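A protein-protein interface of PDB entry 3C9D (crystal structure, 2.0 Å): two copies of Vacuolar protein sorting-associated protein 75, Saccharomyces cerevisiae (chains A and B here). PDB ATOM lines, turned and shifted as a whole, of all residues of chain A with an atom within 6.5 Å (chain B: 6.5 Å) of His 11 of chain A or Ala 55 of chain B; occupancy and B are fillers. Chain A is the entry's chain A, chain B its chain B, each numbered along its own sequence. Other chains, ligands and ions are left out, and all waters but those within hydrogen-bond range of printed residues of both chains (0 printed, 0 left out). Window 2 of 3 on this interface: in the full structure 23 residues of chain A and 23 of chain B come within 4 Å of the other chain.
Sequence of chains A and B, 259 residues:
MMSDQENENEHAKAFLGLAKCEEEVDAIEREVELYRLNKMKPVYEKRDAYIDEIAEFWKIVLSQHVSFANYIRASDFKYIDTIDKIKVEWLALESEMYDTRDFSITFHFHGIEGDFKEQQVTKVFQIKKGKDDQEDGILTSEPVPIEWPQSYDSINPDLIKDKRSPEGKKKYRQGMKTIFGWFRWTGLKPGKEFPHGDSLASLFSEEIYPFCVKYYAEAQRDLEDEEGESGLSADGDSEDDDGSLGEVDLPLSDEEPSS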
ATOM      1  N   GLU A   8       9.907  33.324  22.072  1.00  0.00           N
ATOM      2  CA  GLU A   8       8.440  33.027  22.053  1.00  0.00           C
ATOM      3  C   GLU A   8       8.079  32.074  20.910  1.00  0.00           C
ATOM      4  O   GLU A   8       7.320  31.127  21.103  1.00  0.00           O
ATOM      5  CB  GLU A   8       7.611  34.324  21.977  1.00  0.00           C
ATOM      6  CG  GLU A   8       7.542  34.996  20.586  1.00  0.00           C
ATOM      7  CD  GLU A   8       8.830  35.729  20.188  1.00  0.00           C
ATOM      8  OE1 GLU A   8       9.764  35.817  21.017  1.00  0.00           O
ATOM      9  OE2 GLU A   8       8.902  36.228  19.041  1.00  0.00           O
ATOM     10  N   ASN A   9       8.625  32.341  19.722  1.00  0.00           N
ATOM     11  CA  ASN A   9       8.522  31.413  18.600  1.00  0.00           C
ATOM     12  C   ASN A   9       9.451  30.222  18.792  1.00  0.00           C
ATOM     13  O   ASN A   9       9.105  29.093  18.446  1.00  0.00           O
ATOM     14  CB  ASN A   9       8.810  32.115  17.264  1.00  0.00           C
ATOM     15  CG  ASN A   9       9.147  33.591  17.430  1.00  0.00           C
ATOM     16  OD1 ASN A   9       8.255  34.441  17.455  1.00  0.00           O
ATOM     17  ND2 ASN A   9      10.438  33.903  17.520  1.00  0.00           N
ATOM     18  N   GLU A  10      10.618  30.480  19.383  1.00  0.00           N
ATOM     19  CA  GLU A  10      11.556  29.427  19.765  1.00  0.00           C
ATOM     20  C   GLU A  10      10.931  28.500  20.819  1.00  0.00           C
ATOM     21  O   GLU A  10      11.032  27.271  20.716  1.00  0.00           O
ATOM     22  CB  GLU A  10      12.865  30.035  20.286  1.00  0.00           C
ATOM     23  CG  GLU A  10      13.634  30.884  19.256  1.00  0.00           C
ATOM     24  CD  GLU A  10      13.029  32.278  19.038  1.00  0.00           C
ATOM     25  OE1 GLU A  10      12.039  32.628  19.724  1.00  0.00           O
ATOM     26  OE2 GLU A  10      13.550  33.024  18.177  1.00  0.00           O
ATOM     27  N   HIS A  11      10.247  29.092  21.800  1.00  0.00           N
ATOM     28  CA  HIS A  11       9.544  28.315  22.833  1.00  0.00           C
ATOM     29  C   HIS A  11       8.339  27.556  22.267  1.00  0.00           C
ATOM     30  O   HIS A  11       8.131  26.393  22.600  1.00  0.00           O
ATOM     31  CB  HIS A  11       9.115  29.216  23.995  1.00  0.00           C
ATOM     32  CG  HIS A  11      10.195  29.454  25.011  1.00  0.00           C
ATOM     33  ND1 HIS A  11       9.966  29.385  26.369  1.00  0.00           N
ATOM     34  CD2 HIS A  11      11.507  29.770  24.866  1.00  0.00           C
ATOM     35  CE1 HIS A  11      11.089  29.645  27.018  1.00  0.00           C
ATOM     36  NE2 HIS A  11      12.040  29.883  26.129  1.00  0.00           N
ATOM     37  N   ALA A  12       7.553  28.217  21.412  1.00  0.00           N
ATOM     38  CA  ALA A  12       6.394  27.573  20.777  1.00  0.00           C
ATOM     39  C   ALA A  12       6.829  26.375  19.942  1.00  0.00           C
ATOM     40  O   ALA A  12       6.218  25.309  20.013  1.00  0.00           O
ATOM     41  CB  ALA A  12       5.626  28.561  19.928  1.00  0.00           C
ATOM     42  N   LYS A  13       7.902  26.555  19.171  1.00  0.00           N
ATOM     43  CA  LYS A  13       8.513  25.470  18.408  1.00  0.00           C
ATOM     44  C   LYS A  13       8.893  24.306  19.319  1.00  0.00           C
ATOM     45  O   LYS A  13       8.643  23.148  18.996  1.00  0.00           O
ATOM     46  CB  LYS A  13       9.754  25.975  17.680  1.00  0.00           C
ATOM     47  CG  LYS A  13      10.385  24.969  16.724  1.00  0.00           C
ATOM     48  CD  LYS A  13      11.639  25.549  16.072  1.00  0.00           C
ATOM     49  CE  LYS A  13      11.364  26.920  15.439  1.00  0.00           C
ATOM     50  NZ  LYS A  13      12.642  27.666  15.155  1.00  0.00           N
ATOM     51  N   ALA A  14       9.503  24.629  20.455  1.00  0.00           N
ATOM     52  CA  ALA A  14       9.909  23.622  21.427  1.00  0.00           C
ATOM     53  C   ALA A  14       8.699  22.899  22.023  1.00  0.00           C
ATOM     54  O   ALA A  14       8.720  21.675  22.176  1.00  0.00           O
ATOM     55  CB  ALA A  14      10.757  24.260  22.527  1.00  0.00           C
ATOM     56  N   PHE A  15       7.643  23.658  22.329  1.00  0.00           N
ATOM     57  CA  PHE A  15       6.435  23.101  22.960  1.00  0.00           C
ATOM     58  C   PHE A  15       5.718  22.126  22.033  1.00  0.00           C
ATOM     59  O   PHE A  15       5.185  21.102  22.481  1.00  0.00           O
ATOM     60  CB  PHE A  15       5.458  24.212  23.375  1.00  0.00           C
ATOM     61  CG  PHE A  15       5.980  25.130  24.452  1.00  0.00           C
ATOM     62  CD1 PHE A  15       7.025  24.743  25.285  1.00  0.00           C
ATOM     63  CD2 PHE A  15       5.395  26.382  24.650  1.00  0.00           C
ATOM     64  CE1 PHE A  15       7.499  25.598  26.283  1.00  0.00           C
ATOM     65  CE2 PHE A  15       5.862  27.244  25.646  1.00  0.00           C
ATOM     66  CZ  PHE A  15       6.912  26.848  26.466  1.00  0.00           C
ATOM     67  N   LEU A  16       5.701  22.464  20.745  1.00  0.00           N
ATOM     68  CA  LEU A  16       5.107  21.625  19.713  1.00  0.00           C
ATOM     69  C   LEU A  16       5.913  20.344  19.542  1.00  0.00           C
ATOM     70  O   LEU A  16       5.346  19.255  19.472  1.00  0.00           O
ATOM     71  CB  LEU A  16       5.041  22.392  18.386  1.00  0.00           C
ATOM     72  CG  LEU A  16       4.391  21.730  17.164  1.00  0.00           C
ATOM     73  CD1 LEU A  16       2.968  21.226  17.473  1.00  0.00           C
ATOM     74  CD2 LEU A  16       4.376  22.709  15.997  1.00  0.00           C
ATOM     75  N   ILE B  51      14.013  20.493  24.834  1.00  0.00           N
ATOM     76  CA  ILE B  51      14.206  20.987  26.201  1.00  0.00           C
ATOM     77  C   ILE B  51      15.354  21.997  26.280  1.00  0.00           C
ATOM     78  O   ILE B  51      15.261  23.007  26.993  1.00  0.00           O
ATOM     79  CB  ILE B  51      14.458  19.824  27.198  1.00  0.00           C
ATOM     80  CG1 ILE B  51      13.162  19.041  27.446  1.00  0.00           C
ATOM     81  CG2 ILE B  51      15.043  20.355  28.508  1.00  0.00           C
ATOM     82  CD1 ILE B  51      13.362  17.743  28.216  1.00  0.00           C
ATOM     83  N   ASP B  52      16.428  21.720  25.542  1.00  0.00           N
ATOM     84  CA  ASP B  52      17.581  22.621  25.466  1.00  0.00           C
ATOM     85  C   ASP B  52      17.190  24.036  25.018  1.00  0.00           C
ATOM     86  O   ASP B  52      17.857  25.009  25.372  1.00  0.00           O
ATOM     87  CB  ASP B  52      18.647  22.060  24.518  1.00  0.00           C
ATOM     88  CG  ASP B  52      19.415  20.880  25.118  1.00  0.00           C
ATOM     89  OD1 ASP B  52      19.572  20.819  26.361  1.00  0.00           O
ATOM     90  OD2 ASP B  52      19.873  20.014  24.334  1.00  0.00           O
ATOM     91  N   GLU B  53      16.102  24.138  24.257  1.00  0.00           N
ATOM     92  CA  GLU B  53      15.635  25.435  23.731  1.00  0.00           C
ATOM     93  C   GLU B  53      14.860  26.243  24.783  1.00  0.00           C
ATOM     94  O   GLU B  53      14.521  27.413  24.556  1.00  0.00           O
ATOM     95  CB  GLU B  53      14.786  25.228  22.459  1.00  0.00           C
ATOM     96  CG  GLU B  53      15.507  24.466  21.336  1.00  0.00           C
ATOM     97  CD  GLU B  53      14.590  24.058  20.171  1.00  0.00           C
ATOM     98  OE1 GLU B  53      13.438  24.559  20.093  1.00  0.00           O
ATOM     99  OE2 GLU B  53      15.032  23.231  19.328  1.00  0.00           O
ATOM    100  N   ILE B  54      14.554  25.614  25.937  1.00  0.00           N
ATOM    101  CA  ILE B  54      13.702  26.241  26.966  1.00  0.00           C
ATOM    102  C   ILE B  54      14.475  26.716  28.182  1.00  0.00           C
ATOM    103  O   ILE B  54      15.029  25.931  28.954  1.00  0.00           O
ATOM    104  CB  ILE B  54      12.566  25.329  27.371  1.00  0.00           C
ATOM    105  CG1 ILE B  54      11.701  25.023  26.146  1.00  0.00           C
ATOM    106  CG2 ILE B  54      11.721  25.950  28.465  1.00  0.00           C
ATOM    107  CD1 ILE B  54      10.760  23.847  26.329  1.00  0.00           C
ATOM    108  N   ALA B  55      14.480  28.035  28.274  1.00  0.00           N
ATOM    109  CA  ALA B  55      15.184  28.846  29.276  1.00  0.00           C
ATOM    110  C   ALA B  55      15.466  28.198  30.627  1.00  0.00           C
ATOM    111  O   ALA B  55      16.594  27.795  30.883  1.00  0.00           O
ATOM    112  CB  ALA B  55      14.414  30.129  29.505  1.00  0.00           C
ATOM    113  N   GLU B  56      14.449  28.153  31.469  1.00  0.00           N
ATOM    114  CA  GLU B  56      14.632  27.652  32.824  1.00  0.00           C
ATOM    115  C   GLU B  56      13.843  26.351  33.080  1.00  0.00           C
ATOM    116  O   GLU B  56      13.321  26.106  34.166  1.00  0.00           O
ATOM    117  CB  GLU B  56      14.262  28.747  33.816  1.00  0.00           C
ATOM    118  CG  GLU B  56      15.029  30.046  33.653  1.00  0.00           C
ATOM    119  CD  GLU B  56      14.558  31.180  34.573  1.00  0.00           C
ATOM    120  OE1 GLU B  56      13.550  31.007  35.270  1.00  0.00           O
ATOM    121  OE2 GLU B  56      15.219  32.252  34.570  1.00  0.00           O
ATOM    122  N   PHE B  57      13.784  25.547  32.001  1.00  0.00           N
ATOM    123  CA  PHE B  57      13.055  24.289  32.037  1.00  0.00           C
ATOM    124  C   PHE B  57      13.308  23.523  33.338  1.00  0.00           C
ATOM    125  O   PHE B  57      12.386  23.281  34.103  1.00  0.00           O
ATOM    126  CB  PHE B  57      13.391  23.396  30.833  1.00  0.00           C
ATOM    127  CG  PHE B  57      12.586  22.109  30.776  1.00  0.00           C
ATOM    128  CD1 PHE B  57      11.325  22.057  30.190  1.00  0.00           C
ATOM    129  CD2 PHE B  57      13.123  20.938  31.314  1.00  0.00           C
ATOM    130  CE1 PHE B  57      10.611  20.865  30.145  1.00  0.00           C
ATOM    131  CE2 PHE B  57      12.411  19.736  31.266  1.00  0.00           C
ATOM    132  CZ  PHE B  57      11.164  19.697  30.685  1.00  0.00           C
ATOM    133  N   TRP B  58      14.561  23.151  33.586  1.00  0.00           N
ATOM    134  CA  TRP B  58      14.883  22.309  34.744  1.00  0.00           C
ATOM    135  C   TRP B  58      14.647  22.994  36.081  1.00  0.00           C
ATOM    136  O   TRP B  58      14.175  22.362  37.028  1.00  0.00           O
ATOM    137  CB  TRP B  58      16.304  21.755  34.634  1.00  0.00           C
ATOM    138  CG  TRP B  58      16.410  20.741  33.531  1.00  0.00           C
ATOM    139  CD1 TRP B  58      17.050  20.900  32.333  1.00  0.00           C
ATOM    140  CD2 TRP B  58      15.822  19.432  33.501  1.00  0.00           C
ATOM    141  NE1 TRP B  58      16.910  19.767  31.571  1.00  0.00           N
ATOM    142  CE2 TRP B  58      16.165  18.849  32.264  1.00  0.00           C
ATOM    143  CE3 TRP B  58      15.044  18.688  34.409  1.00  0.00           C
ATOM    144  CZ2 TRP B  58      15.754  17.557  31.901  1.00  0.00           C
ATOM    145  CZ3 TRP B  58      14.640  17.408  34.047  1.00  0.00           C
ATOM    146  CH2 TRP B  58      14.998  16.856  32.807  1.00  0.00           C
ATOM    147  N   ILE B  83      20.761  24.747  37.082  1.00  0.00           N
ATOM    148  CA  ILE B  83      20.786  23.532  36.256  1.00  0.00           C
ATOM    149  C   ILE B  83      20.063  23.815  34.948  1.00  0.00           C
ATOM    150  O   ILE B  83      18.881  24.176  34.946  1.00  0.00           O
ATOM    151  CB  ILE B  83      20.125  22.320  36.969  1.00  0.00           C
ATOM    152  CG1 ILE B  83      20.942  21.907  38.199  1.00  0.00           C
ATOM    153  CG2 ILE B  83      19.965  21.113  35.991  1.00  0.00           C
ATOM    154  CD1 ILE B  83      20.201  20.955  39.163  1.00  0.00           C
ATOM    155  N   ASP B  84      20.788  23.686  33.842  1.00  0.00           N
ATOM    156  CA  ASP B  84      20.224  23.947  32.524  1.00  0.00           C
ATOM    157  C   ASP B  84      20.221  22.690  31.655  1.00  0.00           C
ATOM    158  O   ASP B  84      19.816  22.736  30.492  1.00  0.00           O
ATOM    159  CB  ASP B  84      20.984  25.085  31.829  1.00  0.00           C
ATOM    160  CG  ASP B  84      22.448  24.760  31.604  1.00  0.00           C
ATOM    161  OD1 ASP B  84      22.861  23.617  31.867  1.00  0.00           O
ATOM    162  OD2 ASP B  84      23.192  25.648  31.146  1.00  0.00           O
ATOM    163  N   TYR B 216       6.701  20.331  33.960  1.00  0.00           N
ATOM    164  CA  TYR B 216       6.825  21.667  33.390  1.00  0.00           C
ATOM    165  C   TYR B 216       5.455  22.187  32.932  1.00  0.00           C
ATOM    166  O   TYR B 216       5.108  23.346  33.177  1.00  0.00           O
ATOM    167  CB  TYR B 216       7.844  21.680  32.234  1.00  0.00           C
ATOM    168  CG  TYR B 216       7.983  23.028  31.575  1.00  0.00           C
ATOM    169  CD1 TYR B 216       8.858  23.997  32.082  1.00  0.00           C
ATOM    170  CD2 TYR B 216       7.218  23.355  30.459  1.00  0.00           C
ATOM    171  CE1 TYR B 216       8.962  25.249  31.488  1.00  0.00           C
ATOM    172  CE2 TYR B 216       7.318  24.594  29.861  1.00  0.00           C
ATOM    173  CZ  TYR B 216       8.189  25.536  30.371  1.00  0.00           C
ATOM    174  OH  TYR B 216       8.271  26.763  29.759  1.00  0.00           O
ATOM    175  N   GLN B 220       3.102  25.430  34.282  1.00  0.00           N
ATOM    176  CA  GLN B 220       2.512  26.429  33.390  1.00  0.00           C
ATOM    177  C   GLN B 220       0.987  26.452  33.495  1.00  0.00           C
ATOM    178  O   GLN B 220       0.357  27.481  33.256  1.00  0.00           O
ATOM    179  CB  GLN B 220       2.947  26.198  31.937  1.00  0.00           C
ATOM    180  CG  GLN B 220       4.464  26.162  31.713  1.00  0.00           C
ATOM    181  CD  GLN B 220       5.148  27.490  32.011  1.00  0.00           C
ATOM    182  OE1 GLN B 220       5.068  28.009  33.127  1.00  0.00           O
ATOM    183  NE2 GLN B 220       5.834  28.038  31.014  1.00  0.00           N
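OE1 of Glu 10 of chain A is in hydrogen-bond range of N of Glu 8 of chain A (3.2 Å).
The side-chain amide nitrogen of Asn 9 of chain A sits at hydrogen-bond distance from the side-chain carboxylate of Glu 10 of chain A, 3.0 Å away.
The side-chain amide nitrogen of Gln 220 of chain B lies within hydrogen-bond range of the side-chain hydroxyl of Tyr 216 of chain B (3.0 Å).
O of Glu 10 of chain A touches OE1 of Glu 53 of chain B, 3.7 Å away.
Glu 53 of chain B touches His 11 of chain A (O to NE2, 3.8 Å).
His 11 of chain A touches Ala 55 of chain B (NE2 to N, 3.7 Å).
OE1 of Glu 53 of chain B touches CB of Ala 14 of chain A, 3.6 Å away.
CB of Ala 14 of chain A touches CG1 of Ile 54 of chain B (3.8 Å).
Phe 15 of chain A touches Ile 54 of chain B.
Phe 15 of chain A touches Tyr 216 of chain B (CZ to OH, 3.6 Å).
Of the printed residues of chain B, His 11 of chain A touches Glu 53 (3.8 Å) and Ala 55 (3.7 Å).
Of the printed residues of chain B, Ala 14 of chain A touches Glu 53 (3.6 Å) and Ile 54 (3.8 Å).
Printed residues of chain B within 4 Å of Phe 15 of chain A: Ile 54 and Tyr 216.
Of chain A, only His 11 (3.7 Å) comes within 4 Å of Ala 55 of chain B.
Ile 83 of chain B touches none of the printed residues of chain A.
Hydrophobic or aromatic side chains of chain A that line the printed part of chain B: His 11, Ala 14 and Phe 15.
Hydrophobic or aromatic side chains of chain B within 4 Å of the printed part of chain A: Ile 54 and Tyr 216.
Among the printed residues, 7 pairs touch across the chains.
No position is printed for both chains.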
